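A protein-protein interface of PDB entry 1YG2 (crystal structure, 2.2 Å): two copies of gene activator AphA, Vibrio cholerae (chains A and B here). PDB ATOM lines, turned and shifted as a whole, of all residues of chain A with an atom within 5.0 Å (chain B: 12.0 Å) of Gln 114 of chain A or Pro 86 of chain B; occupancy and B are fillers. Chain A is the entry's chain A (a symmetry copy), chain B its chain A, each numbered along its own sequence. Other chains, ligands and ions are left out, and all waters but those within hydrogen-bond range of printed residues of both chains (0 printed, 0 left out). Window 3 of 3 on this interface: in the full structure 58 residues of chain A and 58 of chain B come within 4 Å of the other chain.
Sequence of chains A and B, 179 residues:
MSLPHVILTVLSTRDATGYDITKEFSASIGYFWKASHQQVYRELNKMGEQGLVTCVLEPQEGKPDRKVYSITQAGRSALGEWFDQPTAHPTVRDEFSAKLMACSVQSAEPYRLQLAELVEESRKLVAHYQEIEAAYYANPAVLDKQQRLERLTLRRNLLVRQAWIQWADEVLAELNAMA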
ATOM      1  N   LYS A  99     -19.384  21.863  14.954  1.00  0.00           N
ATOM      2  CA  LYS A  99     -18.162  21.522  15.676  1.00  0.00           C
ATOM      3  C   LYS A  99     -18.172  20.032  16.024  1.00  0.00           C
ATOM      4  O   LYS A  99     -17.149  19.358  15.940  1.00  0.00           O
ATOM      5  CB  LYS A  99     -18.053  22.337  16.969  1.00  0.00           C
ATOM      6  CG  LYS A  99     -17.852  23.840  16.791  1.00  0.00           C
ATOM      7  CD  LYS A  99     -16.454  24.190  16.336  1.00  0.00           C
ATOM      8  CE  LYS A  99     -16.246  25.717  16.259  1.00  0.00           C
ATOM      9  NZ  LYS A  99     -16.126  26.371  17.598  1.00  0.00           N
ATOM     10  N   PRO A 110     -10.943  20.043  23.346  1.00  0.00           N
ATOM     11  CA  PRO A 110     -11.375  21.442  23.410  1.00  0.00           C
ATOM     12  C   PRO A 110     -12.887  21.591  23.339  1.00  0.00           C
ATOM     13  O   PRO A 110     -13.478  22.355  24.094  1.00  0.00           O
ATOM     14  CB  PRO A 110     -10.696  22.076  22.194  1.00  0.00           C
ATOM     15  CG  PRO A 110      -9.480  21.251  22.015  1.00  0.00           C
ATOM     16  CD  PRO A 110     -10.000  19.851  22.231  1.00  0.00           C
ATOM     17  N   TYR A 111     -13.505  20.857  22.422  1.00  0.00           N
ATOM     18  CA  TYR A 111     -14.946  20.931  22.248  1.00  0.00           C
ATOM     19  C   TYR A 111     -15.698  20.475  23.492  1.00  0.00           C
ATOM     20  O   TYR A 111     -16.571  21.182  23.994  1.00  0.00           O
ATOM     21  CB  TYR A 111     -15.387  20.081  21.054  1.00  0.00           C
ATOM     22  CG  TYR A 111     -16.852  20.254  20.733  1.00  0.00           C
ATOM     23  CD1 TYR A 111     -17.367  21.510  20.424  1.00  0.00           C
ATOM     24  CD2 TYR A 111     -17.732  19.174  20.778  1.00  0.00           C
ATOM     25  CE1 TYR A 111     -18.719  21.691  20.170  1.00  0.00           C
ATOM     26  CE2 TYR A 111     -19.087  19.343  20.524  1.00  0.00           C
ATOM     27  CZ  TYR A 111     -19.573  20.604  20.222  1.00  0.00           C
ATOM     28  OH  TYR A 111     -20.910  20.787  19.968  1.00  0.00           O
ATOM     29  N   ARG A 112     -15.349  19.288  23.975  1.00  0.00           N
ATOM     30  CA  ARG A 112     -15.979  18.706  25.150  1.00  0.00           C
ATOM     31  C   ARG A 112     -15.987  19.655  26.339  1.00  0.00           C
ATOM     32  O   ARG A 112     -16.956  19.707  27.093  1.00  0.00           O
ATOM     33  CB  ARG A 112     -15.262  17.417  25.537  1.00  0.00           C
ATOM     34  CG  ARG A 112     -15.985  16.607  26.581  1.00  0.00           C
ATOM     35  CD  ARG A 112     -15.360  15.229  26.747  1.00  0.00           C
ATOM     36  NE  ARG A 112     -16.245  14.339  27.493  1.00  0.00           N
ATOM     37  CZ  ARG A 112     -16.660  14.568  28.736  1.00  0.00           C
ATOM     38  NH1 ARG A 112     -16.264  15.658  29.382  1.00  0.00           N
ATOM     39  NH2 ARG A 112     -17.492  13.718  29.325  1.00  0.00           N
ATOM     40  N   LEU A 113     -14.906  20.408  26.500  1.00  0.00           N
ATOM     41  CA  LEU A 113     -14.792  21.344  27.605  1.00  0.00           C
ATOM     42  C   LEU A 113     -15.633  22.589  27.365  1.00  0.00           C
ATOM     43  O   LEU A 113     -16.235  23.132  28.290  1.00  0.00           O
ATOM     44  CB  LEU A 113     -13.327  21.731  27.808  1.00  0.00           C
ATOM     45  CG  LEU A 113     -12.381  20.558  28.069  1.00  0.00           C
ATOM     46  CD1 LEU A 113     -10.953  21.077  28.151  1.00  0.00           C
ATOM     47  CD2 LEU A 113     -12.773  19.838  29.357  1.00  0.00           C
ATOM     48  N   GLN A 114     -15.673  23.043  26.119  1.00  0.00           N
ATOM     49  CA  GLN A 114     -16.460  24.220  25.781  1.00  0.00           C
ATOM     50  C   GLN A 114     -17.951  23.899  25.885  1.00  0.00           C
ATOM     51  O   GLN A 114     -18.764  24.766  26.195  1.00  0.00           O
ATOM     52  CB  GLN A 114     -16.117  24.696  24.366  1.00  0.00           C
ATOM     53  CG  GLN A 114     -14.692  25.233  24.232  1.00  0.00           C
ATOM     54  CD  GLN A 114     -14.308  25.568  22.796  1.00  0.00           C
ATOM     55  OE1 GLN A 114     -14.986  26.345  22.118  1.00  0.00           O
ATOM     56  NE2 GLN A 114     -13.208  24.984  22.330  1.00  0.00           N
ATOM     57  N   LEU A 115     -18.301  22.642  25.633  1.00  0.00           N
ATOM     58  CA  LEU A 115     -19.692  22.212  25.699  1.00  0.00           C
ATOM     59  C   LEU A 115     -20.113  22.086  27.164  1.00  0.00           C
ATOM     60  O   LEU A 115     -21.103  22.683  27.591  1.00  0.00           O
ATOM     61  CB  LEU A 115     -19.857  20.868  24.981  1.00  0.00           C
ATOM     62  CG  LEU A 115     -21.274  20.382  24.670  1.00  0.00           C
ATOM     63  CD1 LEU A 115     -21.989  21.387  23.781  1.00  0.00           C
ATOM     64  CD2 LEU A 115     -21.205  19.035  23.979  1.00  0.00           C
ATOM     65  N   ALA A 116     -19.348  21.313  27.930  1.00  0.00           N
ATOM     66  CA  ALA A 116     -19.638  21.114  29.346  1.00  0.00           C
ATOM     67  C   ALA A 116     -19.766  22.464  30.037  1.00  0.00           C
ATOM     68  O   ALA A 116     -20.604  22.645  30.921  1.00  0.00           O
ATOM     69  CB  ALA A 116     -18.534  20.293  29.996  1.00  0.00           C
ATOM     70  N   GLU A 117     -18.939  23.415  29.623  1.00  0.00           N
ATOM     71  CA  GLU A 117     -18.987  24.744  30.206  1.00  0.00           C
ATOM     72  C   GLU A 117     -20.322  25.424  29.934  1.00  0.00           C
ATOM     73  O   GLU A 117     -20.976  25.894  30.860  1.00  0.00           O
ATOM     74  CB  GLU A 117     -17.869  25.625  29.652  1.00  0.00           C
ATOM     75  CG  GLU A 117     -18.017  27.082  30.065  1.00  0.00           C
ATOM     76  CD  GLU A 117     -17.896  28.037  28.894  1.00  0.00           C
ATOM     77  OE1 GLU A 117     -18.055  27.582  27.740  1.00  0.00           O
ATOM     78  OE2 GLU A 117     -17.653  29.243  29.130  1.00  0.00           O
ATOM     79  N   LEU A 118     -20.724  25.481  28.666  1.00  0.00           N
ATOM     80  CA  LEU A 118     -21.983  26.129  28.305  1.00  0.00           C
ATOM     81  C   LEU A 118     -23.223  25.419  28.847  1.00  0.00           C
ATOM     82  O   LEU A 118     -24.301  26.010  28.932  1.00  0.00           O
ATOM     83  CB  LEU A 118     -22.093  26.281  26.782  1.00  0.00           C
ATOM     84  CG  LEU A 118     -21.354  27.474  26.159  1.00  0.00           C
ATOM     85  CD1 LEU A 118     -21.620  27.516  24.665  1.00  0.00           C
ATOM     86  CD2 LEU A 118     -21.825  28.776  26.796  1.00  0.00           C
ATOM     87  N   SER B   2     -18.208  28.325  10.157  1.00  0.00           N
ATOM     88  CA  SER B   2     -19.158  28.741   9.091  1.00  0.00           C
ATOM     89  C   SER B   2     -19.169  27.731   7.941  1.00  0.00           C
ATOM     90  O   SER B   2     -18.621  26.640   8.064  1.00  0.00           O
ATOM     91  CB  SER B   2     -18.785  30.139   8.588  1.00  0.00           C
ATOM     92  OG  SER B   2     -17.388  30.251   8.399  1.00  0.00           O
ATOM     93  N   HIS B   5     -15.973  25.929   6.993  1.00  0.00           N
ATOM     94  CA  HIS B   5     -15.493  24.952   7.968  1.00  0.00           C
ATOM     95  C   HIS B   5     -16.331  23.682   7.882  1.00  0.00           C
ATOM     96  O   HIS B   5     -15.838  22.576   8.099  1.00  0.00           O
ATOM     97  CB  HIS B   5     -15.538  25.523   9.383  1.00  0.00           C
ATOM     98  CG  HIS B   5     -14.831  26.829   9.514  1.00  0.00           C
ATOM     99  ND1 HIS B   5     -15.499  28.039   9.518  1.00  0.00           N
ATOM    100  CD2 HIS B   5     -13.511  27.129   9.546  1.00  0.00           C
ATOM    101  CE1 HIS B   5     -14.620  29.022   9.541  1.00  0.00           C
ATOM    102  NE2 HIS B   5     -13.404  28.496   9.557  1.00  0.00           N
ATOM    103  N   ALA B  78      -6.851  26.085   9.321  1.00  0.00           N
ATOM    104  CA  ALA B  78      -8.032  26.920   9.541  1.00  0.00           C
ATOM    105  C   ALA B  78      -9.139  26.150  10.269  1.00  0.00           C
ATOM    106  O   ALA B  78      -9.856  26.717  11.097  1.00  0.00           O
ATOM    107  CB  ALA B  78      -8.564  27.452   8.201  1.00  0.00           C
ATOM    108  N   LEU B  79      -9.282  24.867   9.947  1.00  0.00           N
ATOM    109  CA  LEU B  79     -10.301  24.034  10.586  1.00  0.00           C
ATOM    110  C   LEU B  79      -9.960  23.913  12.072  1.00  0.00           C
ATOM    111  O   LEU B  79     -10.830  24.033  12.931  1.00  0.00           O
ATOM    112  CB  LEU B  79     -10.349  22.641   9.936  1.00  0.00           C
ATOM    113  CG  LEU B  79     -11.392  21.646  10.454  1.00  0.00           C
ATOM    114  CD1 LEU B  79     -12.804  22.175  10.192  1.00  0.00           C
ATOM    115  CD2 LEU B  79     -11.192  20.299   9.768  1.00  0.00           C
ATOM    116  N   GLY B  80      -8.685  23.680  12.370  1.00  0.00           N
ATOM    117  CA  GLY B  80      -8.259  23.558  13.755  1.00  0.00           C
ATOM    118  C   GLY B  80      -8.462  24.845  14.535  1.00  0.00           C
ATOM    119  O   GLY B  80      -8.906  24.816  15.675  1.00  0.00           O
ATOM    120  N   GLU B  81      -8.147  25.973  13.910  1.00  0.00           N
ATOM    121  CA  GLU B  81      -8.283  27.285  14.532  1.00  0.00           C
ATOM    122  C   GLU B  81      -9.745  27.569  14.838  1.00  0.00           C
ATOM    123  O   GLU B  81     -10.088  28.107  15.890  1.00  0.00           O
ATOM    124  CB  GLU B  81      -7.736  28.334  13.573  1.00  0.00           C
ATOM    125  CG  GLU B  81      -7.733  29.757  14.074  1.00  0.00           C
ATOM    126  CD  GLU B  81      -7.131  30.709  13.045  1.00  0.00           C
ATOM    127  OE1 GLU B  81      -6.006  30.433  12.568  1.00  0.00           O
ATOM    128  OE2 GLU B  81      -7.782  31.723  12.705  1.00  0.00           O
ATOM    129  N   TRP B  82     -10.605  27.208  13.898  1.00  0.00           N
ATOM    130  CA  TRP B  82     -12.038  27.398  14.056  1.00  0.00           C
ATOM    131  C   TRP B  82     -12.507  26.584  15.256  1.00  0.00           C
ATOM    132  O   TRP B  82     -13.200  27.086  16.141  1.00  0.00           O
ATOM    133  CB  TRP B  82     -12.745  26.910  12.797  1.00  0.00           C
ATOM    134  CG  TRP B  82     -14.224  26.761  12.909  1.00  0.00           C
ATOM    135  CD1 TRP B  82     -15.144  27.761  13.043  1.00  0.00           C
ATOM    136  CD2 TRP B  82     -14.963  25.540  12.820  1.00  0.00           C
ATOM    137  NE1 TRP B  82     -16.421  27.236  13.031  1.00  0.00           N
ATOM    138  CE2 TRP B  82     -16.335  25.876  12.894  1.00  0.00           C
ATOM    139  CE3 TRP B  82     -14.601  24.196  12.673  1.00  0.00           C
ATOM    140  CZ2 TRP B  82     -17.347  24.909  12.838  1.00  0.00           C
ATOM    141  CZ3 TRP B  82     -15.608  23.235  12.617  1.00  0.00           C
ATOM    142  CH2 TRP B  82     -16.967  23.600  12.695  1.00  0.00           C
ATOM    143  N   PHE B  83     -12.094  25.325  15.263  1.00  0.00           N
ATOM    144  CA  PHE B  83     -12.447  24.367  16.298  1.00  0.00           C
ATOM    145  C   PHE B  83     -12.053  24.802  17.700  1.00  0.00           C
ATOM    146  O   PHE B  83     -12.814  24.608  18.643  1.00  0.00           O
ATOM    147  CB  PHE B  83     -11.784  23.025  15.994  1.00  0.00           C
ATOM    148  CG  PHE B  83     -12.349  21.876  16.773  1.00  0.00           C
ATOM    149  CD1 PHE B  83     -13.498  21.229  16.337  1.00  0.00           C
ATOM    150  CD2 PHE B  83     -11.743  21.451  17.948  1.00  0.00           C
ATOM    151  CE1 PHE B  83     -14.033  20.167  17.051  1.00  0.00           C
ATOM    152  CE2 PHE B  83     -12.272  20.387  18.672  1.00  0.00           C
ATOM    153  CZ  PHE B  83     -13.425  19.746  18.221  1.00  0.00           C
ATOM    154  N   ASP B  84     -10.862  25.374  17.839  1.00  0.00           N
ATOM    155  CA  ASP B  84     -10.379  25.809  19.145  1.00  0.00           C
ATOM    156  C   ASP B  84     -11.115  27.026  19.671  1.00  0.00           C
ATOM    157  O   ASP B  84     -11.254  27.188  20.882  1.00  0.00           O
ATOM    158  CB  ASP B  84      -8.878  26.116  19.098  1.00  0.00           C
ATOM    159  CG  ASP B  84      -8.044  24.892  18.780  1.00  0.00           C
ATOM    160  OD1 ASP B  84      -8.345  23.812  19.331  1.00  0.00           O
ATOM    161  OD2 ASP B  84      -7.081  25.009  17.989  1.00  0.00           O
ATOM    162  N   GLN B  85     -11.574  27.884  18.768  1.00  0.00           N
ATOM    163  CA  GLN B  85     -12.298  29.081  19.176  1.00  0.00           C
ATOM    164  C   GLN B  85     -13.561  28.702  19.929  1.00  0.00           C
ATOM    165  O   GLN B  85     -14.286  27.786  19.538  1.00  0.00           O
ATOM    166  CB  GLN B  85     -12.677  29.935  17.968  1.00  0.00           C
ATOM    167  CG  GLN B  85     -11.501  30.520  17.224  1.00  0.00           C
ATOM    168  CD  GLN B  85     -11.939  31.482  16.149  1.00  0.00           C
ATOM    169  OE1 GLN B  85     -12.718  31.128  15.261  1.00  0.00           O
ATOM    170  NE2 GLN B  85     -11.443  32.712  16.222  1.00  0.00           N
ATOM    171  N   PRO B  86     -13.847  29.413  21.025  1.00  0.00           N
ATOM    172  CA  PRO B  86     -15.039  29.120  21.814  1.00  0.00           C
ATOM    173  C   PRO B  86     -16.298  29.377  21.009  1.00  0.00           C
ATOM    174  O   PRO B  86     -16.405  30.372  20.296  1.00  0.00           O
ATOM    175  CB  PRO B  86     -14.902  30.067  22.996  1.00  0.00           C
ATOM    176  CG  PRO B  86     -14.275  31.266  22.363  1.00  0.00           C
ATOM    177  CD  PRO B  86     -13.194  30.643  21.506  1.00  0.00           C
ATOM    178  N   THR B  87     -17.238  28.453  21.104  1.00  0.00           N
ATOM    179  CA  THR B  87     -18.504  28.588  20.412  1.00  0.00           C
ATOM    180  C   THR B  87     -19.532  28.864  21.502  1.00  0.00           C
ATOM    181  O   THR B  87     -19.612  28.131  22.487  1.00  0.00           O
ATOM    182  CB  THR B  87     -18.851  27.295  19.651  1.00  0.00           C
ATOM    183  OG1 THR B  87     -20.248  27.282  19.339  1.00  0.00           O
ATOM    184  CG2 THR B  87     -18.499  26.076  20.484  1.00  0.00           C
ATOM    185  N   ALA B  88     -20.301  29.935  21.347  1.00  0.00           N
ATOM    186  CA  ALA B  88     -21.298  30.275  22.355  1.00  0.00           C
ATOM    187  C   ALA B  88     -22.708  30.377  21.784  1.00  0.00           C
ATOM    188  O   ALA B  88     -22.900  30.390  20.569  1.00  0.00           O
ATOM    189  CB  ALA B  88     -20.916  31.584  23.039  1.00  0.00           C
ATOM    190  N   HIS B  89     -23.688  30.444  22.680  1.00  0.00           N
ATOM    191  CA  HIS B  89     -25.087  30.552  22.284  1.00  0.00           C
ATOM    192  C   HIS B  89     -25.364  31.889  21.612  1.00  0.00           C
ATOM    193  O   HIS B  89     -24.880  32.927  22.053  1.00  0.00           O
ATOM    194  CB  HIS B  89     -25.994  30.401  23.506  1.00  0.00           C
ATOM    195  CG  HIS B  89     -26.380  28.985  23.802  1.00  0.00           C
ATOM    196  ND1 HIS B  89     -27.151  28.230  22.942  1.00  0.00           N
ATOM    197  CD2 HIS B  89     -26.119  28.193  24.870  1.00  0.00           C
ATOM    198  CE1 HIS B  89     -27.348  27.035  23.468  1.00  0.00           C
ATOM    199  NE2 HIS B  89     -26.733  26.987  24.637  1.00  0.00           N
ATOM    200  N   PRO B  90     -26.140  31.878  20.520  1.00  0.00           N
ATOM    201  CA  PRO B  90     -26.463  33.123  19.816  1.00  0.00           C
ATOM    202  C   PRO B  90     -27.293  34.024  20.727  1.00  0.00           C
ATOM    203  O   PRO B  90     -28.120  33.533  21.496  1.00  0.00           O
ATOM    204  CB  PRO B  90     -27.264  32.639  18.609  1.00  0.00           C
ATOM    205  CG  PRO B  90     -26.736  31.248  18.379  1.00  0.00           C
ATOM    206  CD  PRO B  90     -26.648  30.710  19.782  1.00  0.00           C
ATOM    207  N   THR B  91     -27.068  35.332  20.644  1.00  0.00           N
ATOM    208  CA  THR B  91     -27.798  36.285  21.470  1.00  0.00           C
ATOM    209  C   THR B  91     -29.298  36.083  21.296  1.00  0.00           C
ATOM    210  O   THR B  91     -29.782  35.867  20.185  1.00  0.00           O
ATOM    211  CB  THR B  91     -27.431  37.739  21.095  1.00  0.00           C
ATOM    212  OG1 THR B  91     -26.013  37.916  21.209  1.00  0.00           O
ATOM    213  CG2 THR B  91     -28.135  38.732  22.022  1.00  0.00           C
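The side-chain amino group of Lys 99 of chain A sits close to the backbone carbonyl oxygen of Trp 82 of chain B, 3.3 Å away. The backbone carbonyl oxygen (O) of Gln 85 of chain B lies close to the side-chain amide oxygen (OE1) of Gln 114 of chain A, at 3.0 Å. NZ of Lys 99 of chain A sits at hydrogen-bond distance from O of Gln 85 of chain B, at 3.0 Å. O of Asp 84 of chain B is in hydrogen-bond range of NE2 of Gln 114 of chain A, at 3.3 Å. OE1 of Gln 114 of chain A is in hydrogen-bond range of N of Thr 87 of chain B (3.2 Å). The side-chain amide oxygen (OE1) of Gln 114 of chain A lies close to the backbone nitrogen (N) of Pro 86 of chain B (3.5 Å).
The side-chain amide nitrogen (NE2) of Gln 114 of chain A lies close to the backbone carbonyl oxygen (O) of Pro 110 of chain A.
Among the printed residues, merely in contact across the chains: Leu 118 of chain A with Thr 87 of chain B (3.0 Å), Lys 99 of chain A with Phe 83 of chain B (3.4 Å), Tyr 111 of chain A with Phe 83 of chain B (3.5 Å), Lys 99 of chain A with Thr 87 of chain B (3.5 Å), Leu 118 of chain A with Ala 88 of chain B (3.6 Å), Gln 114 of chain A with Phe 83 of chain B (3.7 Å) and Pro 110 of chain A with Asp 84 of chain B (3.9 Å).
Printed residues of chain B within 4 Å of Gln 114 of chain A: Phe 83, Asp 84, Gln 85, Pro 86 and Thr 87. Pro 86 of chain B touches just one residue of chain A: Gln 114 (2.8 Å). Pro 110 of chain A touches one residue of chain B. Printed residues of chain B within 4 Å of Tyr 111 of chain A: Phe 83 (3.5 Å). No residue of chain B comes within 4 Å of Leu 113 of chain A. No residue of chain B comes within 4 Å of Leu 115 of chain A. No residue of chain B comes within 4 Å of Ala 116 of chain A. Leu 118 of chain A touches just these residues of chain B: Thr 87 (3.0 Å) and Ala 88 (3.6 Å). Of the printed residues of chain A, Asp 84 of chain B touches Pro 110 and Gln 114. Of the printed residues of chain A, Thr 87 of chain B touches Lys 99 (3.5 Å), Gln 114 (3.2 Å) and Leu 118 (3.0 Å). Arg 112 of chain A touches none of the printed residues of chain B. His 89 of chain B touches none of the printed residues of chain A. The nearest residue of chain B that does not touch Gln 114 of chain A is Trp 82 of chain B (6.3 Å).
Of the 16 printed residues of chain B, 7 touch a printed residue of chain A. Printed residues of chain B that touch a printed residue of chain A: Trp 82, Phe 83, Asp 84, Gln 85, Pro 86, Thr 87 and Ala 88. Hydrophobic or aromatic side chains of chain B that line the printed part of chain A: Trp 82, Phe 83 and Pro 86. Along chain B the printed residues that touch a printed residue of chain A span positions 82 to 88. Hydrophobic or aromatic side chains of chain A that line the printed part of chain B: Pro 110, Tyr 111 and Leu 118.
No position is printed for both chains. Of the 13 pairs that touch across the chains among the printed residues, none has its exchanged pair printed and touching as well.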
